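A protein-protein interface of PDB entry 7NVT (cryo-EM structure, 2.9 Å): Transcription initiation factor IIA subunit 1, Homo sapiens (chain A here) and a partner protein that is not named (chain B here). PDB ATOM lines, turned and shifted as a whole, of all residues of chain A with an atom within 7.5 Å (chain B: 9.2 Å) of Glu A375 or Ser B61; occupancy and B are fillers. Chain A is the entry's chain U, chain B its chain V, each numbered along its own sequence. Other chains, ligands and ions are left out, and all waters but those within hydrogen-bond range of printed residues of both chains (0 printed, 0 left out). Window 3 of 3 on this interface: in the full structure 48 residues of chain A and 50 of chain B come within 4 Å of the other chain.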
ATOM      1  N   ASN A 347       3.260 -21.420   5.188  1.00  0.00           N
ATOM      2  CA  ASN A 347       4.003 -21.707   3.965  1.00  0.00           C
ATOM      3  C   ASN A 347       5.332 -22.402   4.232  1.00  0.00           C
ATOM      4  O   ASN A 347       5.731 -23.303   3.486  1.00  0.00           O
ATOM      5  CB  ASN A 347       4.238 -20.416   3.178  1.00  0.00           C
ATOM      6  CG  ASN A 347       4.420 -20.666   1.692  1.00  0.00           C
ATOM      7  OD1 ASN A 347       4.421 -21.811   1.238  1.00  0.00           O
ATOM      8  ND2 ASN A 347       4.571 -19.593   0.925  1.00  0.00           N
ATOM      9  N   LYS A 348       6.019 -21.992   5.294  1.00  0.00           N
ATOM     10  CA  LYS A 348       7.432 -22.287   5.479  1.00  0.00           C
ATOM     11  C   LYS A 348       7.672 -22.998   6.802  1.00  0.00           C
ATOM     12  O   LYS A 348       7.132 -22.611   7.843  1.00  0.00           O
ATOM     13  CB  LYS A 348       8.263 -20.999   5.442  1.00  0.00           C
ATOM     14  CG  LYS A 348       8.125 -20.194   4.157  1.00  0.00           C
ATOM     15  CD  LYS A 348       9.073 -20.672   3.068  1.00  0.00           C
ATOM     16  CE  LYS A 348       9.756 -19.498   2.382  1.00  0.00           C
ATOM     17  NZ  LYS A 348      10.302 -19.860   1.047  1.00  0.00           N
ATOM     18  N   TRP A 349       8.516 -24.026   6.756  1.00  0.00           N
ATOM     19  CA  TRP A 349       8.892 -24.799   7.931  1.00  0.00           C
ATOM     20  C   TRP A 349      10.216 -24.272   8.464  1.00  0.00           C
ATOM     21  O   TRP A 349      11.214 -24.244   7.737  1.00  0.00           O
ATOM     22  CB  TRP A 349       9.019 -26.287   7.591  1.00  0.00           C
ATOM     23  CG  TRP A 349       7.704 -26.986   7.422  1.00  0.00           C
ATOM     24  CD1 TRP A 349       6.919 -26.995   6.306  1.00  0.00           C
ATOM     25  CD2 TRP A 349       7.024 -27.784   8.398  1.00  0.00           C
ATOM     26  NE1 TRP A 349       5.792 -27.746   6.527  1.00  0.00           N
ATOM     27  CE2 TRP A 349       5.831 -28.242   7.804  1.00  0.00           C
ATOM     28  CE3 TRP A 349       7.307 -28.155   9.716  1.00  0.00           C
ATOM     29  CZ2 TRP A 349       4.922 -29.051   8.482  1.00  0.00           C
ATOM     30  CZ3 TRP A 349       6.402 -28.958  10.388  1.00  0.00           C
ATOM     31  CH2 TRP A 349       5.225 -29.397   9.770  1.00  0.00           C
ATOM     32  N   LYS A 350      10.222 -23.860   9.729  1.00  0.00           N
ATOM     33  CA  LYS A 350      11.426 -23.384  10.400  1.00  0.00           C
ATOM     34  C   LYS A 350      11.875 -24.433  11.404  1.00  0.00           C
ATOM     35  O   LYS A 350      11.073 -24.900  12.220  1.00  0.00           O
ATOM     36  CB  LYS A 350      11.182 -22.047  11.103  1.00  0.00           C
ATOM     37  CG  LYS A 350      12.463 -21.337  11.521  1.00  0.00           C
ATOM     38  CD  LYS A 350      12.211 -19.881  11.878  1.00  0.00           C
ATOM     39  CE  LYS A 350      13.491 -19.186  12.312  1.00  0.00           C
ATOM     40  NZ  LYS A 350      13.260 -17.760  12.675  1.00  0.00           N
ATOM     41  N   PHE A 351      13.153 -24.799  11.341  1.00  0.00           N
ATOM     42  CA  PHE A 351      13.718 -25.862  12.166  1.00  0.00           C
ATOM     43  C   PHE A 351      14.693 -25.249  13.163  1.00  0.00           C
ATOM     44  O   PHE A 351      15.622 -24.532  12.773  1.00  0.00           O
ATOM     45  CB  PHE A 351      14.413 -26.907  11.296  1.00  0.00           C
ATOM     46  CG  PHE A 351      13.648 -27.263  10.053  1.00  0.00           C
ATOM     47  CD1 PHE A 351      12.448 -27.950  10.135  1.00  0.00           C
ATOM     48  CD2 PHE A 351      14.127 -26.908   8.803  1.00  0.00           C
ATOM     49  CE1 PHE A 351      11.743 -28.278   8.992  1.00  0.00           C
ATOM     50  CE2 PHE A 351      13.425 -27.233   7.658  1.00  0.00           C
ATOM     51  CZ  PHE A 351      12.232 -27.919   7.753  1.00  0.00           C
ATOM     52  N   ASP A 373      15.262 -22.966   7.422  1.00  0.00           N
ATOM     53  CA  ASP A 373      13.952 -22.583   6.913  1.00  0.00           C
ATOM     54  C   ASP A 373      13.711 -23.300   5.594  1.00  0.00           C
ATOM     55  O   ASP A 373      14.591 -23.323   4.727  1.00  0.00           O
ATOM     56  CB  ASP A 373      13.852 -21.067   6.722  1.00  0.00           C
ATOM     57  CG  ASP A 373      12.423 -20.564   6.791  1.00  0.00           C
ATOM     58  OD1 ASP A 373      11.496 -21.368   6.556  1.00  0.00           O
ATOM     59  OD2 ASP A 373      12.227 -19.365   7.080  1.00  0.00           O
ATOM     60  N   ALA A 374      12.523 -23.883   5.444  1.00  0.00           N
ATOM     61  CA  ALA A 374      12.182 -24.646   4.253  1.00  0.00           C
ATOM     62  C   ALA A 374      10.788 -24.257   3.784  1.00  0.00           C
ATOM     63  O   ALA A 374       9.960 -23.775   4.560  1.00  0.00           O
ATOM     64  CB  ALA A 374      12.251 -26.157   4.512  1.00  0.00           C
ATOM     65  N   GLU A 375      10.540 -24.477   2.495  1.00  0.00           N
ATOM     66  CA  GLU A 375       9.265 -24.164   1.864  1.00  0.00           C
ATOM     67  C   GLU A 375       8.625 -25.451   1.366  1.00  0.00           C
ATOM     68  O   GLU A 375       9.291 -26.274   0.728  1.00  0.00           O
ATOM     69  CB  GLU A 375       9.451 -23.183   0.704  1.00  0.00           C
ATOM     70  CG  GLU A 375       8.145 -22.672   0.108  1.00  0.00           C
ATOM     71  CD  GLU A 375       7.608 -23.563  -0.997  1.00  0.00           C
ATOM     72  OE1 GLU A 375       8.418 -24.199  -1.704  1.00  0.00           O
ATOM     73  OE2 GLU A 375       6.371 -23.628  -1.159  1.00  0.00           O
ATOM     74  N   TRP A 376       7.339 -25.621   1.659  1.00  0.00           N
ATOM     75  CA  TRP A 376       6.598 -26.799   1.226  1.00  0.00           C
ATOM     76  C   TRP A 376       5.510 -26.417   0.230  1.00  0.00           C
ATOM     77  O   TRP A 376       5.641 -26.658  -0.971  1.00  0.00           O
ATOM     78  CB  TRP A 376       5.981 -27.515   2.429  1.00  0.00           C
ATOM     79  CG  TRP A 376       5.276 -28.787   2.070  1.00  0.00           C
ATOM     80  CD1 TRP A 376       5.845 -29.944   1.626  1.00  0.00           C
ATOM     81  CD2 TRP A 376       3.866 -29.030   2.126  1.00  0.00           C
ATOM     82  NE1 TRP A 376       4.877 -30.893   1.402  1.00  0.00           N
ATOM     83  CE2 TRP A 376       3.653 -30.356   1.700  1.00  0.00           C
ATOM     84  CE3 TRP A 376       2.762 -28.254   2.494  1.00  0.00           C
ATOM     85  CZ2 TRP A 376       2.383 -30.923   1.633  1.00  0.00           C
ATOM     86  CZ3 TRP A 376       1.502 -28.819   2.426  1.00  0.00           C
ATOM     87  CH2 TRP A 376       1.323 -30.141   1.999  1.00  0.00           C
ATOM     88  N   PHE B  58      21.708 -23.996   7.340  1.00  0.00           N
ATOM     89  CA  PHE B  58      21.337 -24.664   6.101  1.00  0.00           C
ATOM     90  C   PHE B  58      19.994 -24.134   5.624  1.00  0.00           C
ATOM     91  O   PHE B  58      19.174 -23.670   6.422  1.00  0.00           O
ATOM     92  CB  PHE B  58      21.271 -26.184   6.284  1.00  0.00           C
ATOM     93  CG  PHE B  58      20.076 -26.649   7.067  1.00  0.00           C
ATOM     94  CD1 PHE B  58      20.005 -26.443   8.436  1.00  0.00           C
ATOM     95  CD2 PHE B  58      19.024 -27.289   6.434  1.00  0.00           C
ATOM     96  CE1 PHE B  58      18.906 -26.870   9.157  1.00  0.00           C
ATOM     97  CE2 PHE B  58      17.923 -27.717   7.152  1.00  0.00           C
ATOM     98  CZ  PHE B  58      17.864 -27.507   8.514  1.00  0.00           C
ATOM     99  N   ARG B  59      19.784 -24.209   4.311  1.00  0.00           N
ATOM    100  CA  ARG B  59      18.525 -23.823   3.687  1.00  0.00           C
ATOM    101  C   ARG B  59      18.169 -24.858   2.632  1.00  0.00           C
ATOM    102  O   ARG B  59      19.057 -25.518   2.088  1.00  0.00           O
ATOM    103  CB  ARG B  59      18.614 -22.430   3.052  1.00  0.00           C
ATOM    104  CG  ARG B  59      19.005 -21.319   4.018  1.00  0.00           C
ATOM    105  CD  ARG B  59      17.795 -20.770   4.759  1.00  0.00           C
ATOM    106  NE  ARG B  59      18.072 -19.467   5.360  1.00  0.00           N
ATOM    107  CZ  ARG B  59      17.179 -18.490   5.502  1.00  0.00           C
ATOM    108  NH1 ARG B  59      15.925 -18.652   5.097  1.00  0.00           N
ATOM    109  NH2 ARG B  59      17.541 -17.344   6.061  1.00  0.00           N
ATOM    110  N   GLY B  60      16.877 -24.997   2.348  1.00  0.00           N
ATOM    111  CA  GLY B  60      16.432 -25.972   1.372  1.00  0.00           C
ATOM    112  C   GLY B  60      14.936 -25.892   1.169  1.00  0.00           C
ATOM    113  O   GLY B  60      14.255 -25.020   1.714  1.00  0.00           O
ATOM    114  N   SER B  61      14.430 -26.820   0.361  1.00  0.00           N
ATOM    115  CA  SER B  61      13.009 -26.926   0.058  1.00  0.00           C
ATOM    116  C   SER B  61      12.472 -28.235   0.620  1.00  0.00           C
ATOM    117  O   SER B  61      13.073 -29.295   0.417  1.00  0.00           O
ATOM    118  CB  SER B  61      12.765 -26.857  -1.452  1.00  0.00           C
ATOM    119  OG  SER B  61      11.392 -27.027  -1.754  1.00  0.00           O
ATOM    120  N   LEU B  62      11.345 -28.156   1.324  1.00  0.00           N
ATOM    121  CA  LEU B  62      10.757 -29.332   1.951  1.00  0.00           C
ATOM    122  C   LEU B  62       9.885 -30.081   0.951  1.00  0.00           C
ATOM    123  O   LEU B  62       9.078 -29.476   0.239  1.00  0.00           O
ATOM    124  CB  LEU B  62       9.933 -28.926   3.172  1.00  0.00           C
ATOM    125  CG  LEU B  62       9.571 -30.047   4.151  1.00  0.00           C
ATOM    126  CD1 LEU B  62       9.505 -29.504   5.568  1.00  0.00           C
ATOM    127  CD2 LEU B  62       8.251 -30.704   3.776  1.00  0.00           C
ATOM    128  N   ASN B  63      10.051 -31.402   0.902  1.00  0.00           N
ATOM    129  CA  ASN B  63       9.276 -32.264   0.019  1.00  0.00           C
ATOM    130  C   ASN B  63       8.287 -33.146   0.768  1.00  0.00           C
ATOM    131  O   ASN B  63       7.183 -33.387   0.272  1.00  0.00           O
ATOM    132  CB  ASN B  63      10.216 -33.149  -0.808  1.00  0.00           C
ATOM    133  CG  ASN B  63       9.468 -34.055  -1.765  1.00  0.00           C
ATOM    134  OD1 ASN B  63       8.432 -33.680  -2.312  1.00  0.00           O
ATOM    135  ND2 ASN B  63       9.994 -35.258  -1.974  1.00  0.00           N
ATOM    136  N   THR B  64       8.655 -33.632   1.952  1.00  0.00           N
ATOM    137  CA  THR B  64       7.779 -34.503   2.722  1.00  0.00           C
ATOM    138  C   THR B  64       8.136 -34.383   4.196  1.00  0.00           C
ATOM    139  O   THR B  64       9.293 -34.151   4.556  1.00  0.00           O
ATOM    140  CB  THR B  64       7.888 -35.961   2.257  1.00  0.00           C
ATOM    141  OG1 THR B  64       7.447 -36.067   0.898  1.00  0.00           O
ATOM    142  CG2 THR B  64       7.045 -36.872   3.134  1.00  0.00           C
ATOM    143  N   TYR B  65       7.123 -34.546   5.044  1.00  0.00           N
ATOM    144  CA  TYR B  65       7.311 -34.483   6.486  1.00  0.00           C
ATOM    145  C   TYR B  65       6.373 -35.477   7.152  1.00  0.00           C
ATOM    146  O   TYR B  65       5.302 -35.799   6.631  1.00  0.00           O
ATOM    147  CB  TYR B  65       7.057 -33.070   7.026  1.00  0.00           C
ATOM    148  CG  TYR B  65       5.593 -32.696   7.095  1.00  0.00           C
ATOM    149  CD1 TYR B  65       4.938 -32.170   5.990  1.00  0.00           C
ATOM    150  CD2 TYR B  65       4.866 -32.865   8.267  1.00  0.00           C
ATOM    151  CE1 TYR B  65       3.600 -31.826   6.048  1.00  0.00           C
ATOM    152  CE2 TYR B  65       3.529 -32.526   8.334  1.00  0.00           C
ATOM    153  CZ  TYR B  65       2.901 -32.005   7.222  1.00  0.00           C
ATOM    154  OH  TYR B  65       1.569 -31.665   7.286  1.00  0.00           O
ATOM    155  N   PHE B  74      11.456 -35.216   8.232  1.00  0.00           N
ATOM    156  CA  PHE B  74      11.495 -34.243   7.149  1.00  0.00           C
ATOM    157  C   PHE B  74      12.348 -34.756   5.996  1.00  0.00           C
ATOM    158  O   PHE B  74      13.423 -35.327   6.195  1.00  0.00           O
ATOM    159  CB  PHE B  74      12.051 -32.908   7.647  1.00  0.00           C
ATOM    160  CG  PHE B  74      11.155 -32.201   8.620  1.00  0.00           C
ATOM    161  CD1 PHE B  74       9.978 -31.612   8.193  1.00  0.00           C
ATOM    162  CD2 PHE B  74      11.492 -32.118   9.960  1.00  0.00           C
ATOM    163  CE1 PHE B  74       9.151 -30.957   9.084  1.00  0.00           C
ATOM    164  CE2 PHE B  74      10.670 -31.465  10.856  1.00  0.00           C
ATOM    165  CZ  PHE B  74       9.498 -30.882  10.416  1.00  0.00           C
ATOM    166  N   VAL B  75      11.854 -34.544   4.779  1.00  0.00           N
ATOM    167  CA  VAL B  75      12.566 -34.893   3.553  1.00  0.00           C
ATOM    168  C   VAL B  75      12.719 -33.598   2.767  1.00  0.00           C
ATOM    169  O   VAL B  75      11.741 -33.077   2.218  1.00  0.00           O
ATOM    170  CB  VAL B  75      11.833 -35.958   2.730  1.00  0.00           C
ATOM    171  CG1 VAL B  75      12.541 -36.187   1.402  1.00  0.00           C
ATOM    172  CG2 VAL B  75      11.727 -37.257   3.517  1.00  0.00           C
ATOM    173  N   LEU B  76      13.940 -33.075   2.707  1.00  0.00           N
ATOM    174  CA  LEU B  76      14.223 -31.814   2.039  1.00  0.00           C
ATOM    175  C   LEU B  76      14.888 -32.072   0.694  1.00  0.00           C
ATOM    176  O   LEU B  76      15.661 -33.024   0.544  1.00  0.00           O
ATOM    177  CB  LEU B  76      15.126 -30.932   2.903  1.00  0.00           C
ATOM    178  CG  LEU B  76      14.588 -30.536   4.280  1.00  0.00           C
ATOM    179  CD1 LEU B  76      15.687 -29.886   5.105  1.00  0.00           C
ATOM    180  CD2 LEU B  76      13.387 -29.613   4.161  1.00  0.00           C
ATOM    181  N   ASN B  77      14.584 -31.220  -0.281  1.00  0.00           N
ATOM    182  CA  ASN B  77      15.146 -31.310  -1.621  1.00  0.00           C
ATOM    183  C   ASN B  77      15.885 -30.021  -1.950  1.00  0.00           C
ATOM    184  O   ASN B  77      15.416 -28.925  -1.627  1.00  0.00           O
ATOM    185  CB  ASN B  77      14.053 -31.566  -2.665  1.00  0.00           C
ATOM    186  CG  ASN B  77      13.408 -32.929  -2.511  1.00  0.00           C
ATOM    187  OD1 ASN B  77      13.327 -33.470  -1.408  1.00  0.00           O
ATOM    188  ND2 ASN B  77      12.945 -33.493  -3.620  1.00  0.00           N
ATOM    189  N   ASP B  78      17.044 -30.159  -2.595  1.00  0.00           N
ATOM    190  CA  ASP B  78      17.879 -29.019  -2.969  1.00  0.00           C
ATOM    191  C   ASP B  78      18.249 -28.194  -1.734  1.00  0.00           C
ATOM    192  O   ASP B  78      17.880 -27.027  -1.593  1.00  0.00           O
ATOM    193  CB  ASP B  78      17.178 -28.154  -4.022  1.00  0.00           C
ATOM    194  CG  ASP B  78      16.970 -28.886  -5.333  1.00  0.00           C
ATOM    195  OD1 ASP B  78      17.781 -29.781  -5.652  1.00  0.00           O
ATOM    196  OD2 ASP B  78      15.994 -28.567  -6.045  1.00  0.00           O
ATOM    197  N   VAL B  79      18.993 -28.833  -0.836  1.00  0.00           N
ATOM    198  CA  VAL B  79      19.383 -28.236   0.437  1.00  0.00           C
ATOM    199  C   VAL B  79      20.800 -27.695   0.316  1.00  0.00           C
ATOM    200  O   VAL B  79      21.703 -28.385  -0.173  1.00  0.00           O
ATOM    201  CB  VAL B  79      19.286 -29.262   1.582  1.00  0.00           C
ATOM    202  CG1 VAL B  79      19.661 -28.617   2.911  1.00  0.00           C
ATOM    203  CG2 VAL B  79      17.893 -29.858   1.645  1.00  0.00           C
ATOM    204  N   GLU B  80      20.993 -26.456   0.763  1.00  0.00           N
ATOM    205  CA  GLU B  80      22.307 -25.825   0.800  1.00  0.00           C
ATOM    206  C   GLU B  80      22.699 -25.630   2.256  1.00  0.00           C
ATOM    207  O   GLU B  80      21.980 -24.966   3.010  1.00  0.00           O
ATOM    208  CB  GLU B  80      22.298 -24.485   0.053  1.00  0.00           C
ATOM    209  CG  GLU B  80      23.473 -23.568   0.375  1.00  0.00           C
ATOM    210  CD  GLU B  80      23.395 -22.243  -0.357  1.00  0.00           C
ATOM    211  OE1 GLU B  80      22.310 -21.624  -0.355  1.00  0.00           O
ATOM    212  OE2 GLU B  80      24.420 -21.818  -0.932  1.00  0.00           O
ATOM    213  N   VAL B  90      23.638 -30.445  -1.469  1.00  0.00           N
ATOM    214  CA  VAL B  90      23.107 -31.804  -1.523  1.00  0.00           C
ATOM    215  C   VAL B  90      21.739 -31.762  -2.189  1.00  0.00           C
ATOM    216  O   VAL B  90      20.928 -30.873  -1.912  1.00  0.00           O
ATOM    217  CB  VAL B  90      23.017 -32.435  -0.117  1.00  0.00           C
ATOM    218  CG1 VAL B  90      22.218 -31.542   0.819  1.00  0.00           C
ATOM    219  CG2 VAL B  90      22.403 -33.826  -0.195  1.00  0.00           C
ATOM    220  N   ASP B  91      21.487 -32.731  -3.072  1.00  0.00           N
ATOM    221  CA  ASP B  91      20.222 -32.756  -3.801  1.00  0.00           C
ATOM    222  C   ASP B  91      19.058 -33.110  -2.882  1.00  0.00           C
ATOM    223  O   ASP B  91      18.010 -32.455  -2.914  1.00  0.00           O
ATOM    224  CB  ASP B  91      20.312 -33.747  -4.963  1.00  0.00           C
ATOM    225  CG  ASP B  91      19.121 -33.659  -5.898  1.00  0.00           C
ATOM    226  OD1 ASP B  91      18.000 -34.007  -5.471  1.00  0.00           O
ATOM    227  OD2 ASP B  91      19.307 -33.240  -7.059  1.00  0.00           O
ATOM    228  N   LYS B  92      19.222 -34.144  -2.059  1.00  0.00           N
ATOM    229  CA  LYS B  92      18.157 -34.612  -1.184  1.00  0.00           C
ATOM    230  C   LYS B  92      18.745 -35.048   0.149  1.00  0.00           C
ATOM    231  O   LYS B  92      19.829 -35.636   0.195  1.00  0.00           O
ATOM    232  CB  LYS B  92      17.383 -35.774  -1.818  1.00  0.00           C
ATOM    233  CG  LYS B  92      16.202 -36.259  -0.989  1.00  0.00           C
ATOM    234  CD  LYS B  92      15.236 -37.096  -1.816  1.00  0.00           C
ATOM    235  CE  LYS B  92      15.813 -38.466  -2.144  1.00  0.00           C
ATOM    236  NZ  LYS B  92      15.769 -39.387  -0.975  1.00  0.00           N
ATOM    237  N   VAL B  93      18.022 -34.757   1.229  1.00  0.00           N
ATOM    238  CA  VAL B  93      18.442 -35.118   2.577  1.00  0.00           C
ATOM    239  C   VAL B  93      17.215 -35.506   3.390  1.00  0.00           C
ATOM    240  O   VAL B  93      16.133 -34.935   3.230  1.00  0.00           O
ATOM    241  CB  VAL B  93      19.203 -33.965   3.271  1.00  0.00           C
ATOM    242  CG1 VAL B  93      19.407 -34.270   4.749  1.00  0.00           C
ATOM    243  CG2 VAL B  93      20.534 -33.726   2.587  1.00  0.00           C
ATOM    244  N   ILE B  95      15.974 -35.833   7.339  1.00  0.00           N
ATOM    245  CA  ILE B  95      16.281 -35.368   8.685  1.00  0.00           C
ATOM    246  C   ILE B  95      15.405 -36.162   9.645  1.00  0.00           C
ATOM    247  O   ILE B  95      14.173 -36.143   9.545  1.00  0.00           O
ATOM    248  CB  ILE B  95      16.056 -33.859   8.837  1.00  0.00           C
ATOM    249  CG1 ILE B  95      17.043 -33.084   7.960  1.00  0.00           C
ATOM    250  CG2 ILE B  95      16.204 -33.445  10.296  1.00  0.00           C
ATOM    251  CD1 ILE B  95      16.635 -31.651   7.703  1.00  0.00           C
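OG of Ser B61 sits at hydrogen-bond distance from O of Glu A375. The backbone carbonyl oxygen (O) of Glu A375 lies within hydrogen-bond range of the backbone NH (N) of Leu B62 (2.8 Å). The backbone carbonyl oxygen of Asp A373 sits close to the backbone carbonyl oxygen of Gly B60.
The backbone carbonyl oxygen (O) of Asn A347 is in hydrogen-bond range of the backbone NH (N) of Trp A376 (3.4 Å). The backbone NH (N) of Trp A349 is in hydrogen-bond range of the backbone carbonyl oxygen (O) of Ala A374 (2.6 Å). O of Arg B59 lies within hydrogen-bond range of N of Glu B80. The backbone carbonyl oxygen of Ser B61 is in hydrogen-bond range of the backbone NH of Asn B77 (2.5 Å). N of Ile B95 lies within hydrogen-bond range of O of Phe B74 (2.8 Å). The backbone carbonyl oxygen (O) of Val B93 sits at hydrogen-bond distance from the backbone NH (N) of Leu B76 (2.9 Å).
Phe B74 touches Trp A349 (CE1 to CE3, 3.4 Å). CD2 of Phe A351 touches CZ of Phe B58, at 3.8 Å. Phe A351 touches Phe B74. CB of Asp A373 touches NH1 of Arg B59, at 3.6 Å. CA of Ala A374 touches O of Gly B60, 3.3 Å away. Ala A374 touches Leu B62. Leu B76 touches Ala A374. Glu A375 touches Gly B60 (N to O, 3.8 Å). Trp A376 touches Leu B62. Trp A376 touches Asn B63 (NE1 to O, 3.6 Å).
Of chain B, only Gly B60, Ser B61 and Leu B62 come within 4 Å of Glu A375. Ser B61 touches just one residue of chain A: Glu A375 (3.3 Å). Of chain B, only Gly B60, Leu B62 and Leu B76 come within 4 Å of Ala A374. Printed residues of chain A within 4 Å of Phe B58: Phe A351. Of the printed residues of chain A, Gly B60 touches Asp A373, Ala A374 and Glu A375. Of the printed residues of chain B, Phe A351 touches Phe B58 (3.8 Å), Leu B62 (3.8 Å) and Phe B74 (3.7 Å). Of the printed residues of chain B, Trp A349 touches Leu B62 (3.6 Å), Tyr B65 (3.7 Å) and Phe B74 (3.4 Å). Glu B80 touches none of the printed residues of chain A. The nearest residue of chain B that does not touch Glu A375 is Asn B63 (5.2 Å).
Hydrophobic or aromatic side chains of chain B that line the printed part of chain A: Phe B58, Leu B62, Tyr B65, Phe B74 and Leu B76. Hydrophobic or aromatic side chains of chain A within 4 Å of the printed part of chain B: Trp A349, Phe A351, Ala A374 and Trp A376. Among the printed residues, no Asp or Glu carboxylate lies within 4 Å of a Lys or Arg side-chain nitrogen of the other chain.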
